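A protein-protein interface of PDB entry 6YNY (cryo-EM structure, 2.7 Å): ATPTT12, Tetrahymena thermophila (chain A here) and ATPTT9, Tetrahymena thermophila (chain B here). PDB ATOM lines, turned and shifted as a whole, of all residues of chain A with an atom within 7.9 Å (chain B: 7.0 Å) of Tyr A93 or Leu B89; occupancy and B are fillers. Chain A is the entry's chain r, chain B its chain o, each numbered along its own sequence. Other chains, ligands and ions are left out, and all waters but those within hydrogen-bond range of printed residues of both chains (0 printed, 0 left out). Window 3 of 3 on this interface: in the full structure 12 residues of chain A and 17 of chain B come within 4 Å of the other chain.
O of Pro B87 lies within hydrogen-bond range of ND2 of Asn B92, 3.4 Å away.
N of Thr B88 lies within hydrogen-bond range of OE1 of Glu B91, 3.3 Å away.
The backbone carbonyl oxygen (O) of Asn B92 sits close to the side-chain amide nitrogen (ND2) of Asn B96, 3.1 Å away.
The side-chain hydroxyl (OH) of Tyr A93 sits at hydrogen-bond distance from the guanidinium group (NH2) of Arg A97 (3.2 Å).
Asn A90 touches Pro B87.
OD1 of Asn A90 touches CA of Thr B88, 3.3 Å away.
Tyr A93 touches Leu B89.
C of Gly B86 touches OH of Tyr A94, at 3.1 Å.
Asn B92 touches Tyr A94.
Tyr A93 touches just one residue of chain B: Leu B89.
Leu B89 touches just one residue of chain A: Tyr A93 (3.7 Å).
Of the printed residues of chain A, Thr B88 touches Asn A90 (3.3 Å).
Printed residues of chain B within 4 Å of Tyr A94: Gly B86, Pro B87 and Asn B92.
The nearest printed residue of chain A that does not touch Thr B88 is Tyr A94 (4.6 Å).
The side-chain hydroxyl of Tyr A94 sits at hydrogen-bond distance from the backbone carbonyl oxygen of Pro B87 (2.4 Å).
O of Gly B86 is in hydrogen-bond range of ND2 of Asn A90.
Of the 11 printed residues of chain B, 5 touch a printed residue of chain A.
Printed residues of chain A that touch a printed residue of chain B: Asn A90, Tyr A93 and Tyr A94.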
ATOM      1  N   MET A  84     -28.988 -15.494  38.019  1.00  0.00           N
ATOM      2  CA  MET A  84     -29.690 -15.291  36.763  1.00  0.00           C
ATOM      3  C   MET A  84     -29.836 -16.633  36.069  1.00  0.00           C
ATOM      4  O   MET A  84     -28.878 -17.406  35.997  1.00  0.00           O
ATOM      5  CB  MET A  84     -28.956 -14.293  35.864  1.00  0.00           C
ATOM      6  CG  MET A  84     -27.546 -14.673  35.519  1.00  0.00           C
ATOM      7  SD  MET A  84     -26.706 -13.354  34.631  1.00  0.00           S
ATOM      8  CE  MET A  84     -25.073 -14.047  34.488  1.00  0.00           C
ATOM      9  N   GLN A  85     -31.034 -16.904  35.570  1.00  0.00           N
ATOM     10  CA  GLN A  85     -31.384 -18.189  34.991  1.00  0.00           C
ATOM     11  C   GLN A  85     -31.910 -17.999  33.575  1.00  0.00           C
ATOM     12  O   GLN A  85     -32.097 -16.879  33.096  1.00  0.00           O
ATOM     13  CB  GLN A  85     -32.412 -18.912  35.872  1.00  0.00           C
ATOM     14  CG  GLN A  85     -33.572 -18.056  36.314  1.00  0.00           C
ATOM     15  CD  GLN A  85     -34.385 -18.702  37.416  1.00  0.00           C
ATOM     16  OE1 GLN A  85     -33.861 -19.474  38.216  1.00  0.00           O
ATOM     17  NE2 GLN A  85     -35.672 -18.388  37.464  1.00  0.00           N
ATOM     18  N   THR A  86     -32.146 -19.121  32.902  1.00  0.00           N
ATOM     19  CA  THR A  86     -32.518 -19.100  31.497  1.00  0.00           C
ATOM     20  C   THR A  86     -33.241 -20.389  31.147  1.00  0.00           C
ATOM     21  O   THR A  86     -33.084 -21.413  31.814  1.00  0.00           O
ATOM     22  CB  THR A  86     -31.288 -18.926  30.602  1.00  0.00           C
ATOM     23  OG1 THR A  86     -31.680 -18.961  29.225  1.00  0.00           O
ATOM     24  CG2 THR A  86     -30.276 -20.024  30.863  1.00  0.00           C
ATOM     25  N   ASN A  88     -33.011 -21.324  27.797  1.00  0.00           N
ATOM     26  CA  ASN A  88     -32.340 -21.750  26.581  1.00  0.00           C
ATOM     27  C   ASN A  88     -31.603 -23.060  26.801  1.00  0.00           C
ATOM     28  O   ASN A  88     -30.972 -23.272  27.840  1.00  0.00           O
ATOM     29  CB  ASN A  88     -31.355 -20.684  26.111  1.00  0.00           C
ATOM     30  CG  ASN A  88     -32.037 -19.432  25.634  1.00  0.00           C
ATOM     31  OD1 ASN A  88     -33.257 -19.299  25.712  1.00  0.00           O
ATOM     32  ND2 ASN A  88     -31.248 -18.496  25.141  1.00  0.00           N
ATOM     33  N   SER A  89     -31.690 -23.942  25.814  1.00  0.00           N
ATOM     34  CA  SER A  89     -30.922 -25.171  25.833  1.00  0.00           C
ATOM     35  C   SER A  89     -29.461 -24.867  25.521  1.00  0.00           C
ATOM     36  O   SER A  89     -29.077 -23.729  25.240  1.00  0.00           O
ATOM     37  CB  SER A  89     -31.496 -26.165  24.832  1.00  0.00           C
ATOM     38  OG  SER A  89     -31.369 -25.684  23.509  1.00  0.00           O
ATOM     39  N   ASN A  90     -28.629 -25.904  25.573  1.00  0.00           N
ATOM     40  CA  ASN A  90     -27.224 -25.718  25.241  1.00  0.00           C
ATOM     41  C   ASN A  90     -27.044 -25.397  23.764  1.00  0.00           C
ATOM     42  O   ASN A  90     -26.142 -24.635  23.404  1.00  0.00           O
ATOM     43  CB  ASN A  90     -26.429 -26.960  25.629  1.00  0.00           C
ATOM     44  CG  ASN A  90     -24.944 -26.715  25.641  1.00  0.00           C
ATOM     45  OD1 ASN A  90     -24.441 -25.942  26.451  1.00  0.00           O
ATOM     46  ND2 ASN A  90     -24.229 -27.382  24.750  1.00  0.00           N
ATOM     47  N   TYR A  91     -27.893 -25.953  22.899  1.00  0.00           N
ATOM     48  CA  TYR A  91     -27.826 -25.616  21.483  1.00  0.00           C
ATOM     49  C   TYR A  91     -28.256 -24.176  21.243  1.00  0.00           C
ATOM     50  O   TYR A  91     -27.647 -23.468  20.435  1.00  0.00           O
ATOM     51  CB  TYR A  91     -28.694 -26.573  20.671  1.00  0.00           C
ATOM     52  CG  TYR A  91     -28.817 -26.199  19.214  1.00  0.00           C
ATOM     53  CD1 TYR A  91     -27.882 -26.628  18.287  1.00  0.00           C
ATOM     54  CD2 TYR A  91     -29.870 -25.418  18.765  1.00  0.00           C
ATOM     55  CE1 TYR A  91     -27.989 -26.289  16.959  1.00  0.00           C
ATOM     56  CE2 TYR A  91     -29.986 -25.072  17.440  1.00  0.00           C
ATOM     57  CZ  TYR A  91     -29.044 -25.510  16.539  1.00  0.00           C
ATOM     58  OH  TYR A  91     -29.162 -25.165  15.215  1.00  0.00           O
ATOM     59  N   ASP A  92     -29.309 -23.730  21.929  1.00  0.00           N
ATOM     60  CA  ASP A  92     -29.760 -22.355  21.769  1.00  0.00           C
ATOM     61  C   ASP A  92     -28.680 -21.366  22.175  1.00  0.00           C
ATOM     62  O   ASP A  92     -28.558 -20.295  21.573  1.00  0.00           O
ATOM     63  CB  ASP A  92     -31.026 -22.119  22.589  1.00  0.00           C
ATOM     64  CG  ASP A  92     -32.188 -22.975  22.133  1.00  0.00           C
ATOM     65  OD1 ASP A  92     -31.998 -23.802  21.220  1.00  0.00           O
ATOM     66  OD2 ASP A  92     -33.296 -22.818  22.686  1.00  0.00           O
ATOM     67  N   TYR A  93     -27.883 -21.711  23.186  1.00  0.00           N
ATOM     68  CA  TYR A  93     -26.840 -20.809  23.654  1.00  0.00           C
ATOM     69  C   TYR A  93     -25.715 -20.693  22.634  1.00  0.00           C
ATOM     70  O   TYR A  93     -25.302 -19.586  22.274  1.00  0.00           O
ATOM     71  CB  TYR A  93     -26.304 -21.294  24.999  1.00  0.00           C
ATOM     72  CG  TYR A  93     -25.205 -20.436  25.572  1.00  0.00           C
ATOM     73  CD1 TYR A  93     -25.487 -19.213  26.155  1.00  0.00           C
ATOM     74  CD2 TYR A  93     -23.887 -20.854  25.536  1.00  0.00           C
ATOM     75  CE1 TYR A  93     -24.486 -18.429  26.679  1.00  0.00           C
ATOM     76  CE2 TYR A  93     -22.881 -20.078  26.058  1.00  0.00           C
ATOM     77  CZ  TYR A  93     -23.185 -18.866  26.629  1.00  0.00           C
ATOM     78  OH  TYR A  93     -22.181 -18.090  27.153  1.00  0.00           O
ATOM     79  N   TYR A  94     -25.207 -21.828  22.155  1.00  0.00           N
ATOM     80  CA  TYR A  94     -24.125 -21.798  21.180  1.00  0.00           C
ATOM     81  C   TYR A  94     -24.596 -21.344  19.808  1.00  0.00           C
ATOM     82  O   TYR A  94     -23.768 -20.935  18.988  1.00  0.00           O
ATOM     83  CB  TYR A  94     -23.469 -23.173  21.094  1.00  0.00           C
ATOM     84  CG  TYR A  94     -22.578 -23.471  22.270  1.00  0.00           C
ATOM     85  CD1 TYR A  94     -21.230 -23.155  22.242  1.00  0.00           C
ATOM     86  CD2 TYR A  94     -23.087 -24.051  23.416  1.00  0.00           C
ATOM     87  CE1 TYR A  94     -20.418 -23.417  23.319  1.00  0.00           C
ATOM     88  CE2 TYR A  94     -22.284 -24.317  24.496  1.00  0.00           C
ATOM     89  CZ  TYR A  94     -20.948 -23.999  24.444  1.00  0.00           C
ATOM     90  OH  TYR A  94     -20.143 -24.266  25.524  1.00  0.00           O
ATOM     91  N   TYR A  95     -25.898 -21.409  19.537  1.00  0.00           N
ATOM     92  CA  TYR A  95     -26.432 -20.782  18.335  1.00  0.00           C
ATOM     93  C   TYR A  95     -26.353 -19.266  18.432  1.00  0.00           C
ATOM     94  O   TYR A  95     -25.973 -18.594  17.469  1.00  0.00           O
ATOM     95  CB  TYR A  95     -27.875 -21.229  18.115  1.00  0.00           C
ATOM     96  CG  TYR A  95     -28.621 -20.433  17.070  1.00  0.00           C
ATOM     97  CD1 TYR A  95     -28.675 -20.856  15.755  1.00  0.00           C
ATOM     98  CD2 TYR A  95     -29.276 -19.260  17.402  1.00  0.00           C
ATOM     99  CE1 TYR A  95     -29.353 -20.133  14.807  1.00  0.00           C
ATOM    100  CE2 TYR A  95     -29.950 -18.532  16.462  1.00  0.00           C
ATOM    101  CZ  TYR A  95     -29.991 -18.972  15.164  1.00  0.00           C
ATOM    102  OH  TYR A  95     -30.669 -18.245  14.221  1.00  0.00           O
ATOM    103  N   ASN A  96     -26.712 -18.712  19.590  1.00  0.00           N
ATOM    104  CA  ASN A  96     -26.672 -17.268  19.768  1.00  0.00           C
ATOM    105  C   ASN A  96     -25.246 -16.744  19.715  1.00  0.00           C
ATOM    106  O   ASN A  96     -24.991 -15.677  19.147  1.00  0.00           O
ATOM    107  CB  ASN A  96     -27.336 -16.890  21.085  1.00  0.00           C
ATOM    108  CG  ASN A  96     -28.806 -17.220  21.108  1.00  0.00           C
ATOM    109  OD1 ASN A  96     -29.427 -17.414  20.068  1.00  0.00           O
ATOM    110  ND2 ASN A  96     -29.373 -17.276  22.297  1.00  0.00           N
ATOM    111  N   ARG A  97     -24.302 -17.476  20.305  1.00  0.00           N
ATOM    112  CA  ARG A  97     -22.903 -17.079  20.220  1.00  0.00           C
ATOM    113  C   ARG A  97     -22.445 -16.997  18.772  1.00  0.00           C
ATOM    114  O   ARG A  97     -21.828 -16.011  18.357  1.00  0.00           O
ATOM    115  CB  ARG A  97     -22.032 -18.059  20.999  1.00  0.00           C
ATOM    116  CG  ARG A  97     -22.063 -17.882  22.498  1.00  0.00           C
ATOM    117  CD  ARG A  97     -21.494 -16.549  22.907  1.00  0.00           C
ATOM    118  NE  ARG A  97     -21.215 -16.482  24.333  1.00  0.00           N
ATOM    119  CZ  ARG A  97     -20.889 -15.368  24.977  1.00  0.00           C
ATOM    120  NH1 ARG A  97     -20.807 -14.219  24.328  1.00  0.00           N
ATOM    121  NH2 ARG A  97     -20.647 -15.402  26.276  1.00  0.00           N
ATOM    122  N   GLN A  98     -22.738 -18.030  17.985  1.00  0.00           N
ATOM    123  CA  GLN A  98     -22.371 -18.000  16.577  1.00  0.00           C
ATOM    124  C   GLN A  98     -23.160 -16.941  15.823  1.00  0.00           C
ATOM    125  O   GLN A  98     -22.682 -16.412  14.815  1.00  0.00           O
ATOM    126  CB  GLN A  98     -22.585 -19.376  15.955  1.00  0.00           C
ATOM    127  CG  GLN A  98     -22.025 -19.519  14.564  1.00  0.00           C
ATOM    128  CD  GLN A  98     -20.529 -19.368  14.516  1.00  0.00           C
ATOM    129  OE1 GLN A  98     -19.848 -19.468  15.533  1.00  0.00           O
ATOM    130  NE2 GLN A  98     -20.005 -19.122  13.328  1.00  0.00           N
ATOM    131  N   PHE A  99     -24.366 -16.624  16.292  1.00  0.00           N
ATOM    132  CA  PHE A  99     -25.113 -15.515  15.717  1.00  0.00           C
ATOM    133  C   PHE A  99     -24.421 -14.188  15.984  1.00  0.00           C
ATOM    134  O   PHE A  99     -24.491 -13.275  15.157  1.00  0.00           O
ATOM    135  CB  PHE A  99     -26.532 -15.498  16.277  1.00  0.00           C
ATOM    136  CG  PHE A  99     -27.479 -14.652  15.493  1.00  0.00           C
ATOM    137  CD1 PHE A  99     -28.301 -15.219  14.547  1.00  0.00           C
ATOM    138  CD2 PHE A  99     -27.544 -13.290  15.697  1.00  0.00           C
ATOM    139  CE1 PHE A  99     -29.170 -14.450  13.821  1.00  0.00           C
ATOM    140  CE2 PHE A  99     -28.411 -12.517  14.972  1.00  0.00           C
ATOM    141  CZ  PHE A  99     -29.226 -13.097  14.032  1.00  0.00           C
ATOM    142  N   GLN A 100     -23.752 -14.064  17.131  1.00  0.00           N
ATOM    143  CA  GLN A 100     -22.983 -12.862  17.421  1.00  0.00           C
ATOM    144  C   GLN A 100     -21.745 -12.777  16.539  1.00  0.00           C
ATOM    145  O   GLN A 100     -21.439 -11.718  15.982  1.00  0.00           O
ATOM    146  CB  GLN A 100     -22.587 -12.843  18.893  1.00  0.00           C
ATOM    147  CG  GLN A 100     -23.737 -12.741  19.853  1.00  0.00           C
ATOM    148  CD  GLN A 100     -23.305 -12.931  21.283  1.00  0.00           C
ATOM    149  OE1 GLN A 100     -22.415 -13.726  21.575  1.00  0.00           O
ATOM    150  NE2 GLN A 100     -23.923 -12.192  22.187  1.00  0.00           N
ATOM    151  N   ARG A 101     -21.015 -13.886  16.409  1.00  0.00           N
ATOM    152  CA  ARG A 101     -19.846 -13.898  15.539  1.00  0.00           C
ATOM    153  C   ARG A 101     -20.225 -13.602  14.097  1.00  0.00           C
ATOM    154  O   ARG A 101     -19.455 -12.966  13.371  1.00  0.00           O
ATOM    155  CB  ARG A 101     -19.140 -15.249  15.628  1.00  0.00           C
ATOM    156  CG  ARG A 101     -18.786 -15.670  17.029  1.00  0.00           C
ATOM    157  CD  ARG A 101     -17.957 -16.932  17.043  1.00  0.00           C
ATOM    158  NE  ARG A 101     -17.861 -17.506  18.383  1.00  0.00           N
ATOM    159  CZ  ARG A 101     -18.612 -18.503  18.839  1.00  0.00           C
ATOM    160  NH1 ARG A 101     -19.528 -19.069  18.069  1.00  0.00           N
ATOM    161  NH2 ARG A 101     -18.443 -18.941  20.076  1.00  0.00           N
ATOM    162  N   ASP A 146     -15.425 -14.425  22.743  1.00  0.00           N
ATOM    163  CA  ASP A 146     -16.821 -14.133  23.042  1.00  0.00           C
ATOM    164  C   ASP A 146     -16.971 -12.888  23.905  1.00  0.00           C
ATOM    165  O   ASP A 146     -17.968 -12.167  23.785  1.00  0.00           O
ATOM    166  CB  ASP A 146     -17.462 -15.333  23.734  1.00  0.00           C
ATOM    167  CG  ASP A 146     -17.458 -16.573  22.869  1.00  0.00           C
ATOM    168  OD1 ASP A 146     -17.103 -16.466  21.677  1.00  0.00           O
ATOM    169  OD2 ASP A 146     -17.805 -17.657  23.382  1.00  0.00           O
ATOM    170  N   GLY B  86     -20.436 -26.714  22.594  1.00  0.00           N
ATOM    171  CA  GLY B  86     -19.443 -26.863  23.624  1.00  0.00           C
ATOM    172  C   GLY B  86     -20.058 -27.333  24.924  1.00  0.00           C
ATOM    173  O   GLY B  86     -21.217 -27.755  24.975  1.00  0.00           O
ATOM    174  N   PRO B  87     -19.285 -27.278  26.001  1.00  0.00           N
ATOM    175  CA  PRO B  87     -19.813 -27.678  27.306  1.00  0.00           C
ATOM    176  C   PRO B  87     -20.856 -26.697  27.814  1.00  0.00           C
ATOM    177  O   PRO B  87     -20.884 -25.521  27.450  1.00  0.00           O
ATOM    178  CB  PRO B  87     -18.569 -27.686  28.199  1.00  0.00           C
ATOM    179  CG  PRO B  87     -17.644 -26.744  27.546  1.00  0.00           C
ATOM    180  CD  PRO B  87     -17.865 -26.907  26.080  1.00  0.00           C
ATOM    181  N   THR B  88     -21.726 -27.210  28.678  1.00  0.00           N
ATOM    182  CA  THR B  88     -22.809 -26.414  29.223  1.00  0.00           C
ATOM    183  C   THR B  88     -22.275 -25.348  30.177  1.00  0.00           C
ATOM    184  O   THR B  88     -21.120 -25.375  30.610  1.00  0.00           O
ATOM    185  CB  THR B  88     -23.811 -27.305  29.950  1.00  0.00           C
ATOM    186  OG1 THR B  88     -23.168 -27.946  31.055  1.00  0.00           O
ATOM    187  CG2 THR B  88     -24.356 -28.354  29.018  1.00  0.00           C
ATOM    188  N   LEU B  89     -23.149 -24.393  30.500  1.00  0.00           N
ATOM    189  CA  LEU B  89     -22.786 -23.338  31.438  1.00  0.00           C
ATOM    190  C   LEU B  89     -22.391 -23.908  32.789  1.00  0.00           C
ATOM    191  O   LEU B  89     -21.531 -23.345  33.475  1.00  0.00           O
ATOM    192  CB  LEU B  89     -23.949 -22.364  31.601  1.00  0.00           C
ATOM    193  CG  LEU B  89     -24.451 -21.687  30.328  1.00  0.00           C
ATOM    194  CD1 LEU B  89     -25.642 -20.815  30.639  1.00  0.00           C
ATOM    195  CD2 LEU B  89     -23.352 -20.877  29.687  1.00  0.00           C
ATOM    196  N   GLU B  90     -23.011 -25.017  33.191  1.00  0.00           N
ATOM    197  CA  GLU B  90     -22.669 -25.639  34.462  1.00  0.00           C
ATOM    198  C   GLU B  90     -21.320 -26.343  34.395  1.00  0.00           C
ATOM    199  O   GLU B  90     -20.633 -26.458  35.413  1.00  0.00           O
ATOM    200  CB  GLU B  90     -23.767 -26.620  34.866  1.00  0.00           C
ATOM    201  CG  GLU B  90     -23.559 -27.262  36.223  1.00  0.00           C
ATOM    202  CD  GLU B  90     -24.706 -28.167  36.618  1.00  0.00           C
ATOM    203  OE1 GLU B  90     -25.667 -28.288  35.830  1.00  0.00           O
ATOM    204  OE2 GLU B  90     -24.649 -28.758  37.715  1.00  0.00           O
ATOM    205  N   GLU B  91     -20.927 -26.816  33.213  1.00  0.00           N
ATOM    206  CA  GLU B  91     -19.633 -27.470  33.067  1.00  0.00           C
ATOM    207  C   GLU B  91     -18.500 -26.453  33.045  1.00  0.00           C
ATOM    208  O   GLU B  91     -17.497 -26.616  33.747  1.00  0.00           O
ATOM    209  CB  GLU B  91     -19.621 -28.313  31.794  1.00  0.00           C
ATOM    210  CG  GLU B  91     -20.541 -29.512  31.847  1.00  0.00           C
ATOM    211  CD  GLU B  91     -20.671 -30.211  30.509  1.00  0.00           C
ATOM    212  OE1 GLU B  91     -19.967 -29.815  29.558  1.00  0.00           O
ATOM    213  OE2 GLU B  91     -21.481 -31.155  30.406  1.00  0.00           O
ATOM    214  N   ASN B  92     -18.640 -25.398  32.239  1.00  0.00           N
ATOM    215  CA  ASN B  92     -17.636 -24.341  32.233  1.00  0.00           C
ATOM    216  C   ASN B  92     -17.527 -23.679  33.597  1.00  0.00           C
ATOM    217  O   ASN B  92     -16.443 -23.237  33.989  1.00  0.00           O
ATOM    218  CB  ASN B  92     -17.968 -23.306  31.161  1.00  0.00           C
ATOM    219  CG  ASN B  92     -17.722 -23.820  29.764  1.00  0.00           C
ATOM    220  OD1 ASN B  92     -16.772 -24.564  29.523  1.00  0.00           O
ATOM    221  ND2 ASN B  92     -18.578 -23.428  28.832  1.00  0.00           N
ATOM    222  N   HIS B  93     -18.637 -23.600  34.329  1.00  0.00           N
ATOM    223  CA  HIS B  93     -18.602 -23.050  35.677  1.00  0.00           C
ATOM    224  C   HIS B  93     -17.685 -23.870  36.571  1.00  0.00           C
ATOM    225  O   HIS B  93     -16.761 -23.336  37.193  1.00  0.00           O
ATOM    226  CB  HIS B  93     -20.016 -23.005  36.248  1.00  0.00           C
ATOM    227  CG  HIS B  93     -20.092 -22.465  37.640  1.00  0.00           C
ATOM    228  ND1 HIS B  93     -20.488 -23.232  38.714  1.00  0.00           N
ATOM    229  CD2 HIS B  93     -19.825 -21.234  38.134  1.00  0.00           C
ATOM    230  CE1 HIS B  93     -20.461 -22.496  39.810  1.00  0.00           C
ATOM    231  NE2 HIS B  93     -20.063 -21.280  39.485  1.00  0.00           N
ATOM    232  N   ILE B  94     -17.918 -25.181  36.632  1.00  0.00           N
ATOM    233  CA  ILE B  94     -17.070 -26.051  37.439  1.00  0.00           C
ATOM    234  C   ILE B  94     -15.632 -25.993  36.952  1.00  0.00           C
ATOM    235  O   ILE B  94     -14.689 -25.996  37.753  1.00  0.00           O
ATOM    236  CB  ILE B  94     -17.620 -27.486  37.413  1.00  0.00           C
ATOM    237  CG1 ILE B  94     -19.009 -27.523  38.047  1.00  0.00           C
ATOM    238  CG2 ILE B  94     -16.674 -28.426  38.123  1.00  0.00           C
ATOM    239  CD1 ILE B  94     -19.736 -28.819  37.841  1.00  0.00           C
ATOM    240  N   THR B  95     -15.439 -25.945  35.635  1.00  0.00           N
ATOM    241  CA  THR B  95     -14.092 -25.845  35.089  1.00  0.00           C
ATOM    242  C   THR B  95     -13.398 -24.579  35.567  1.00  0.00           C
ATOM    243  O   THR B  95     -12.200 -24.592  35.871  1.00  0.00           O
ATOM    244  CB  THR B  95     -14.147 -25.880  33.565  1.00  0.00           C
ATOM    245  OG1 THR B  95     -14.573 -27.175  33.129  1.00  0.00           O
ATOM    246  CG2 THR B  95     -12.795 -25.562  32.971  1.00  0.00           C
ATOM    247  N   ASN B  96     -14.136 -23.473  35.642  1.00  0.00           N
ATOM    248  CA  ASN B  96     -13.550 -22.214  36.082  1.00  0.00           C
ATOM    249  C   ASN B  96     -13.338 -22.186  37.590  1.00  0.00           C
ATOM    250  O   ASN B  96     -12.355 -21.610  38.067  1.00  0.00           O
ATOM    251  CB  ASN B  96     -14.436 -21.050  35.648  1.00  0.00           C
ATOM    252  CG  ASN B  96     -14.570 -20.950  34.147  1.00  0.00           C
ATOM    253  OD1 ASN B  96     -13.732 -21.454  33.401  1.00  0.00           O
ATOM    254  ND2 ASN B  96     -15.625 -20.290  33.693  1.00  0.00           N
